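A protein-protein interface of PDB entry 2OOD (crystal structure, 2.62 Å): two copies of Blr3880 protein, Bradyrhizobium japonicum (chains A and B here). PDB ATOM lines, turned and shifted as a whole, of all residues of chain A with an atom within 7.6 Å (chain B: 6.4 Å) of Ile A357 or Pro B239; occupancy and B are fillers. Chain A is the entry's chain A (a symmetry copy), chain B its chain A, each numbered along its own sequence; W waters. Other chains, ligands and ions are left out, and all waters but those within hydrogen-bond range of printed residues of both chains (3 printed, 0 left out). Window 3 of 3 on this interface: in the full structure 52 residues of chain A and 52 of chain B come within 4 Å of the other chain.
OE1 of Gln B94 sits close to OD1 of Asn B238 (3.1 Å).
OH of Tyr B276 sits at hydrogen-bond distance from O of Ser B304, 2.7 Å away.
OG of Ser B243 lies within hydrogen-bond range of O of Pro B239 (3.4 Å).
N of Tyr B276 is in hydrogen-bond range of O of Ser B236.
The backbone NH (N) of Ser A356 sits at hydrogen-bond distance from the side-chain carboxylate (OD1) of Asp A354.
Of the printed residues of chain B, Ser A356 touches Pro B239 (3.1 Å).
Ile A357 touches two residues of chain B.
Pro B239 touches just these residues of chain A: Thr A351 (3.8 Å), Ser A356 (3.1 Å) and Ile A357 (3.9 Å).
Printed residues of chain A within 4 Å of Tyr B276: Ile A357.
The nearest residue of chain B that does not touch Ile A357 is Ser B304 (6.2 Å).
The nearest residue of chain A that does not touch Pro B239 is Asp A354 (5.7 Å).
NE2 of Gln B94 sits at hydrogen-bond distance from OD2 of Asp A354 (2.9 Å).
The side-chain hydroxyl (OG1) of Thr A351 sits at hydrogen-bond distance from the backbone carbonyl oxygen (O) of Gly B303 (2.9 Å).
OE1 of Gln B94 sits close to OG1 of Thr A351 (3.3 Å).
Of the 13 printed residues of chain B, 4 touch a printed residue of chain A.
Hydrophobic or aromatic side chains of chain B that line the printed part of chain A: Pro B239 and Tyr B276.
Of the 12 printed residues of chain A, 5 touch a printed residue of chain B.
Printed residues of chain A that touch a printed residue of chain B: Cys A348, Thr A351, Asp A354, Ser A356 and Ile A357.
Among the printed residues, no Asp or Glu carboxylate lies within 4 Å of a Lys or Arg side-chain nitrogen of the other chain.
CA of Gly B303 touches N of Cys A348, 3.8 Å away.
Pro B239 touches Thr A351 (CG to CG2, 3.8 Å).
OG of Ser A356 touches CG of Pro B239 (3.1 Å).
Ile A357 touches Pro B239.
Tyr B276 touches Ile A357.
No position is printed for both chains.
Water W1 lies within hydrogen-bond range of OG of Ser B243 (2.6 Å) and O of Ser A356 (3.2 Å).
Water W3 lies within hydrogen-bond range of the side-chain amide oxygen (OE1) of Gln B94, the side-chain hydroxyl (OG) of Ser A356, the side-chain amide nitrogen (ND2) of Asn B238 and the side-chain carboxylate (OD2) of Asp A354.
Water W2 lies within hydrogen-bond range of O of Cys A348 (2.8 Å) and O of Gly B303 (2.8 Å).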
ATOM      1  N   CYS A 348     -19.612  15.881 -26.681  1.00  0.00           N
ATOM      2  CA  CYS A 348     -19.265  17.097 -27.390  1.00  0.00           C
ATOM      3  C   CYS A 348     -20.076  17.114 -28.673  1.00  0.00           C
ATOM      4  O   CYS A 348     -20.460  18.179 -29.143  1.00  0.00           O
ATOM      5  CB  CYS A 348     -17.770  17.142 -27.705  1.00  0.00           C
ATOM      6  SG  CYS A 348     -16.734  17.454 -26.267  1.00  0.00           S
ATOM      7  N   THR A 351     -23.730  18.365 -28.190  1.00  0.00           N
ATOM      8  CA  THR A 351     -23.860  19.811 -28.154  1.00  0.00           C
ATOM      9  C   THR A 351     -23.841  20.402 -29.557  1.00  0.00           C
ATOM     10  O   THR A 351     -24.470  21.421 -29.812  1.00  0.00           O
ATOM     11  CB  THR A 351     -22.737  20.436 -27.297  1.00  0.00           C
ATOM     12  OG1 THR A 351     -22.824  19.922 -25.964  1.00  0.00           O
ATOM     13  CG2 THR A 351     -22.868  21.947 -27.246  1.00  0.00           C
ATOM     14  N   LEU A 352     -23.135  19.751 -30.474  1.00  0.00           N
ATOM     15  CA  LEU A 352     -23.053  20.227 -31.855  1.00  0.00           C
ATOM     16  C   LEU A 352     -24.310  19.910 -32.676  1.00  0.00           C
ATOM     17  O   LEU A 352     -24.565  20.542 -33.698  1.00  0.00           O
ATOM     18  CB  LEU A 352     -21.844  19.601 -32.556  1.00  0.00           C
ATOM     19  CG  LEU A 352     -20.457  19.923 -32.006  1.00  0.00           C
ATOM     20  CD1 LEU A 352     -19.420  19.103 -32.753  1.00  0.00           C
ATOM     21  CD2 LEU A 352     -20.175  21.410 -32.134  1.00  0.00           C
ATOM     22  N   LEU A 353     -25.092  18.939 -32.216  1.00  0.00           N
ATOM     23  CA  LEU A 353     -26.284  18.504 -32.927  1.00  0.00           C
ATOM     24  C   LEU A 353     -27.621  18.851 -32.288  1.00  0.00           C
ATOM     25  O   LEU A 353     -28.656  18.379 -32.754  1.00  0.00           O
ATOM     26  CB  LEU A 353     -26.221  16.990 -33.136  1.00  0.00           C
ATOM     27  CG  LEU A 353     -25.040  16.507 -33.978  1.00  0.00           C
ATOM     28  CD1 LEU A 353     -24.898  14.998 -33.891  1.00  0.00           C
ATOM     29  CD2 LEU A 353     -25.244  16.957 -35.411  1.00  0.00           C
ATOM     30  N   ASP A 354     -27.629  19.667 -31.240  1.00  0.00           N
ATOM     31  CA  ASP A 354     -28.903  19.984 -30.607  1.00  0.00           C
ATOM     32  C   ASP A 354     -29.475  21.358 -30.971  1.00  0.00           C
ATOM     33  O   ASP A 354     -30.531  21.751 -30.474  1.00  0.00           O
ATOM     34  CB  ASP A 354     -28.794  19.839 -29.084  1.00  0.00           C
ATOM     35  CG  ASP A 354     -28.057  20.987 -28.436  1.00  0.00           C
ATOM     36  OD1 ASP A 354     -27.498  21.830 -29.167  1.00  0.00           O
ATOM     37  OD2 ASP A 354     -28.036  21.041 -27.189  1.00  0.00           O
ATOM     38  N   GLY A 355     -28.780  22.076 -31.845  1.00  0.00           N
ATOM     39  CA  GLY A 355     -29.249  23.382 -32.264  1.00  0.00           C
ATOM     40  C   GLY A 355     -28.967  24.535 -31.314  1.00  0.00           C
ATOM     41  O   GLY A 355     -29.310  25.679 -31.615  1.00  0.00           O
ATOM     42  N   SER A 356     -28.348  24.261 -30.171  1.00  0.00           N
ATOM     43  CA  SER A 356     -28.053  25.330 -29.221  1.00  0.00           C
ATOM     44  C   SER A 356     -27.065  26.321 -29.837  1.00  0.00           C
ATOM     45  O   SER A 356     -26.967  27.462 -29.390  1.00  0.00           O
ATOM     46  CB  SER A 356     -27.497  24.760 -27.909  1.00  0.00           C
ATOM     47  OG  SER A 356     -26.265  24.086 -28.103  1.00  0.00           O
ATOM     48  N   ILE A 357     -26.339  25.886 -30.863  1.00  0.00           N
ATOM     49  CA  ILE A 357     -25.394  26.769 -31.535  1.00  0.00           C
ATOM     50  C   ILE A 357     -25.938  27.095 -32.924  1.00  0.00           C
ATOM     51  O   ILE A 357     -26.488  28.181 -33.129  1.00  0.00           O
ATOM     52  CB  ILE A 357     -23.990  26.133 -31.668  1.00  0.00           C
ATOM     53  CG1 ILE A 357     -23.386  25.892 -30.282  1.00  0.00           C
ATOM     54  CG2 ILE A 357     -23.066  27.064 -32.416  1.00  0.00           C
ATOM     55  CD1 ILE A 357     -22.026  25.215 -30.317  1.00  0.00           C
ATOM     56  N   ASP A 358     -25.793  26.166 -33.871  1.00  0.00           N
ATOM     57  CA  ASP A 358     -26.300  26.372 -35.237  1.00  0.00           C
ATOM     58  C   ASP A 358     -27.545  25.511 -35.483  1.00  0.00           C
ATOM     59  O   ASP A 358     -27.438  24.317 -35.764  1.00  0.00           O
ATOM     60  CB  ASP A 358     -25.227  26.019 -36.269  1.00  0.00           C
ATOM     61  CG  ASP A 358     -25.723  26.185 -37.692  1.00  0.00           C
ATOM     62  OD1 ASP A 358     -26.931  26.472 -37.861  1.00  0.00           O
ATOM     63  OD2 ASP A 358     -24.919  26.027 -38.633  1.00  0.00           O
ATOM     64  N   PRO A 359     -28.742  26.119 -35.422  1.00  0.00           N
ATOM     65  CA  PRO A 359     -29.984  25.371 -35.628  1.00  0.00           C
ATOM     66  C   PRO A 359     -30.161  24.628 -36.944  1.00  0.00           C
ATOM     67  O   PRO A 359     -30.959  23.691 -37.017  1.00  0.00           O
ATOM     68  CB  PRO A 359     -31.066  26.423 -35.387  1.00  0.00           C
ATOM     69  CG  PRO A 359     -30.418  27.672 -35.819  1.00  0.00           C
ATOM     70  CD  PRO A 359     -29.019  27.556 -35.270  1.00  0.00           C
ATOM     71  N   SER A 360     -29.418  25.014 -37.976  1.00  0.00           N
ATOM     72  CA  SER A 360     -29.563  24.330 -39.257  1.00  0.00           C
ATOM     73  C   SER A 360     -28.848  22.981 -39.240  1.00  0.00           C
ATOM     74  O   SER A 360     -29.123  22.115 -40.074  1.00  0.00           O
ATOM     75  CB  SER A 360     -29.043  25.199 -40.414  1.00  0.00           C
ATOM     76  OG  SER A 360     -27.630  25.220 -40.473  1.00  0.00           O
ATOM     77  N   ARG A 361     -27.941  22.797 -38.283  1.00  0.00           N
ATOM     78  CA  ARG A 361     -27.201  21.542 -38.170  1.00  0.00           C
ATOM     79  C   ARG A 361     -27.792  20.597 -37.141  1.00  0.00           C
ATOM     80  O   ARG A 361     -27.259  19.519 -36.907  1.00  0.00           O
ATOM     81  CB  ARG A 361     -25.736  21.817 -37.841  1.00  0.00           C
ATOM     82  CG  ARG A 361     -24.969  22.304 -39.047  1.00  0.00           C
ATOM     83  CD  ARG A 361     -23.485  22.455 -38.787  1.00  0.00           C
ATOM     84  NE  ARG A 361     -22.766  22.635 -40.049  1.00  0.00           N
ATOM     85  CZ  ARG A 361     -21.638  23.337 -40.196  1.00  0.00           C
ATOM     86  NH1 ARG A 361     -21.074  23.942 -39.146  1.00  0.00           N
ATOM     87  NH2 ARG A 361     -21.083  23.450 -41.405  1.00  0.00           N
ATOM     88  N   GLN B  94     -26.065  17.659 -20.522  1.00  0.00           N
ATOM     89  CA  GLN B  94     -25.186  18.802 -20.720  1.00  0.00           C
ATOM     90  C   GLN B  94     -25.339  19.609 -19.429  1.00  0.00           C
ATOM     91  O   GLN B  94     -26.133  19.252 -18.554  1.00  0.00           O
ATOM     92  CB  GLN B  94     -25.632  19.663 -21.908  1.00  0.00           C
ATOM     93  CG  GLN B  94     -25.192  19.179 -23.278  1.00  0.00           C
ATOM     94  CD  GLN B  94     -25.694  20.090 -24.389  1.00  0.00           C
ATOM     95  OE1 GLN B  94     -25.423  21.295 -24.390  1.00  0.00           O
ATOM     96  NE2 GLN B  94     -26.431  19.520 -25.337  1.00  0.00           N
ATOM     97  N   SER B 236     -19.471  31.714 -19.330  1.00  0.00           N
ATOM     98  CA  SER B 236     -19.479  31.157 -20.684  1.00  0.00           C
ATOM     99  C   SER B 236     -19.118  29.680 -20.838  1.00  0.00           C
ATOM    100  O   SER B 236     -18.299  29.334 -21.691  1.00  0.00           O
ATOM    101  CB  SER B 236     -18.522  31.969 -21.549  1.00  0.00           C
ATOM    102  OG  SER B 236     -18.756  33.350 -21.372  1.00  0.00           O
ATOM    103  N   GLU B 237     -19.739  28.800 -20.062  1.00  0.00           N
ATOM    104  CA  GLU B 237     -19.399  27.386 -20.155  1.00  0.00           C
ATOM    105  C   GLU B 237     -20.203  26.558 -21.156  1.00  0.00           C
ATOM    106  O   GLU B 237     -19.663  25.638 -21.774  1.00  0.00           O
ATOM    107  CB  GLU B 237     -19.500  26.736 -18.770  1.00  0.00           C
ATOM    108  CG  GLU B 237     -19.517  25.207 -18.789  1.00  0.00           C
ATOM    109  CD  GLU B 237     -19.701  24.598 -17.403  1.00  0.00           C
ATOM    110  OE1 GLU B 237     -20.409  25.206 -16.567  1.00  0.00           O
ATOM    111  OE2 GLU B 237     -19.149  23.505 -17.152  1.00  0.00           O
ATOM    112  N   ASN B 238     -21.477  26.886 -21.326  1.00  0.00           N
ATOM    113  CA  ASN B 238     -22.347  26.132 -22.224  1.00  0.00           C
ATOM    114  C   ASN B 238     -23.139  27.079 -23.136  1.00  0.00           C
ATOM    115  O   ASN B 238     -23.475  28.195 -22.736  1.00  0.00           O
ATOM    116  CB  ASN B 238     -23.305  25.288 -21.369  1.00  0.00           C
ATOM    117  CG  ASN B 238     -24.242  24.424 -22.196  1.00  0.00           C
ATOM    118  OD1 ASN B 238     -23.899  23.302 -22.585  1.00  0.00           O
ATOM    119  ND2 ASN B 238     -25.435  24.946 -22.474  1.00  0.00           N
ATOM    120  N   PRO B 239     -23.439  26.653 -24.380  1.00  0.00           N
ATOM    121  CA  PRO B 239     -24.200  27.539 -25.271  1.00  0.00           C
ATOM    122  C   PRO B 239     -25.584  27.872 -24.707  1.00  0.00           C
ATOM    123  O   PRO B 239     -25.953  29.051 -24.615  1.00  0.00           O
ATOM    124  CB  PRO B 239     -24.256  26.757 -26.591  1.00  0.00           C
ATOM    125  CG  PRO B 239     -24.130  25.329 -26.152  1.00  0.00           C
ATOM    126  CD  PRO B 239     -23.072  25.407 -25.071  1.00  0.00           C
ATOM    127  N   ALA B 240     -26.343  26.847 -24.320  1.00  0.00           N
ATOM    128  CA  ALA B 240     -27.669  27.081 -23.757  1.00  0.00           C
ATOM    129  C   ALA B 240     -27.562  28.007 -22.532  1.00  0.00           C
ATOM    130  O   ALA B 240     -28.405  28.878 -22.323  1.00  0.00           O
ATOM    131  CB  ALA B 240     -28.318  25.754 -23.366  1.00  0.00           C
ATOM    132  N   GLU B 241     -26.520  27.811 -21.729  1.00  0.00           N
ATOM    133  CA  GLU B 241     -26.295  28.623 -20.538  1.00  0.00           C
ATOM    134  C   GLU B 241     -26.035  30.074 -20.949  1.00  0.00           C
ATOM    135  O   GLU B 241     -26.531  31.002 -20.323  1.00  0.00           O
ATOM    136  CB  GLU B 241     -25.089  28.084 -19.749  1.00  0.00           C
ATOM    137  CG  GLU B 241     -24.774  28.851 -18.465  1.00  0.00           C
ATOM    138  CD  GLU B 241     -23.274  29.022 -18.219  1.00  0.00           C
ATOM    139  OE1 GLU B 241     -22.902  29.580 -17.159  1.00  0.00           O
ATOM    140  OE2 GLU B 241     -22.469  28.610 -19.087  1.00  0.00           O
ATOM    141  N   CYS B 242     -25.250  30.265 -22.002  1.00  0.00           N
ATOM    142  CA  CYS B 242     -24.931  31.610 -22.477  1.00  0.00           C
ATOM    143  C   CYS B 242     -26.167  32.351 -22.962  1.00  0.00           C
ATOM    144  O   CYS B 242     -26.323  33.549 -22.703  1.00  0.00           O
ATOM    145  CB  CYS B 242     -23.894  31.549 -23.601  1.00  0.00           C
ATOM    146  SG  CYS B 242     -22.221  31.252 -23.006  1.00  0.00           S
ATOM    147  N   SER B 243     -27.035  31.637 -23.678  1.00  0.00           N
ATOM    148  CA  SER B 243     -28.274  32.215 -24.190  1.00  0.00           C
ATOM    149  C   SER B 243     -29.156  32.657 -23.016  1.00  0.00           C
ATOM    150  O   SER B 243     -29.604  33.814 -22.962  1.00  0.00           O
ATOM    151  CB  SER B 243     -29.027  31.191 -25.051  1.00  0.00           C
ATOM    152  OG  SER B 243     -28.287  30.855 -26.217  1.00  0.00           O
ATOM    153  N   GLY B 244     -29.387  31.738 -22.074  1.00  0.00           N
ATOM    154  CA  GLY B 244     -30.206  32.040 -20.910  1.00  0.00           C
ATOM    155  C   GLY B 244     -29.731  33.259 -20.131  1.00  0.00           C
ATOM    156  O   GLY B 244     -30.538  34.101 -19.727  1.00  0.00           O
ATOM    157  N   TYR B 276     -16.809  29.695 -24.155  1.00  0.00           N
ATOM    158  CA  TYR B 276     -17.521  30.547 -25.099  1.00  0.00           C
ATOM    159  C   TYR B 276     -17.267  32.047 -24.999  1.00  0.00           C
ATOM    160  O   TYR B 276     -18.120  32.852 -25.367  1.00  0.00           O
ATOM    161  CB  TYR B 276     -19.018  30.248 -25.024  1.00  0.00           C
ATOM    162  CG  TYR B 276     -19.339  28.887 -25.592  1.00  0.00           C
ATOM    163  CD1 TYR B 276     -19.285  28.655 -26.959  1.00  0.00           C
ATOM    164  CD2 TYR B 276     -19.608  27.811 -24.762  1.00  0.00           C
ATOM    165  CE1 TYR B 276     -19.481  27.382 -27.488  1.00  0.00           C
ATOM    166  CE2 TYR B 276     -19.807  26.531 -25.280  1.00  0.00           C
ATOM    167  CZ  TYR B 276     -19.737  26.323 -26.645  1.00  0.00           C
ATOM    168  OH  TYR B 276     -19.883  25.050 -27.168  1.00  0.00           O
ATOM    169  N   GLY B 303     -19.768  18.039 -22.507  1.00  0.00           N
ATOM    170  CA  GLY B 303     -19.950  18.414 -23.894  1.00  0.00           C
ATOM    171  C   GLY B 303     -19.819  19.896 -24.165  1.00  0.00           C
ATOM    172  O   GLY B 303     -20.075  20.347 -25.276  1.00  0.00           O
ATOM    173  N   SER B 304     -19.412  20.652 -23.150  1.00  0.00           N
ATOM    174  CA  SER B 304     -19.250  22.098 -23.265  1.00  0.00           C
ATOM    175  C   SER B 304     -18.477  22.492 -24.507  1.00  0.00           C
ATOM    176  O   SER B 304     -18.905  23.374 -25.251  1.00  0.00           O
ATOM    177  CB  SER B 304     -18.539  22.650 -22.031  1.00  0.00           C
ATOM    178  OG  SER B 304     -19.278  22.355 -20.857  1.00  0.00           O
HETATM  179  O   HOH W   1     -28.664  28.343 -26.776  1.00  0.00           O
HETATM  180  O   HOH W   2     -19.418  20.510 -28.008  1.00  0.00           O
HETATM  181  O   HOH W   3     -26.718  23.460 -25.177  1.00  0.00           O
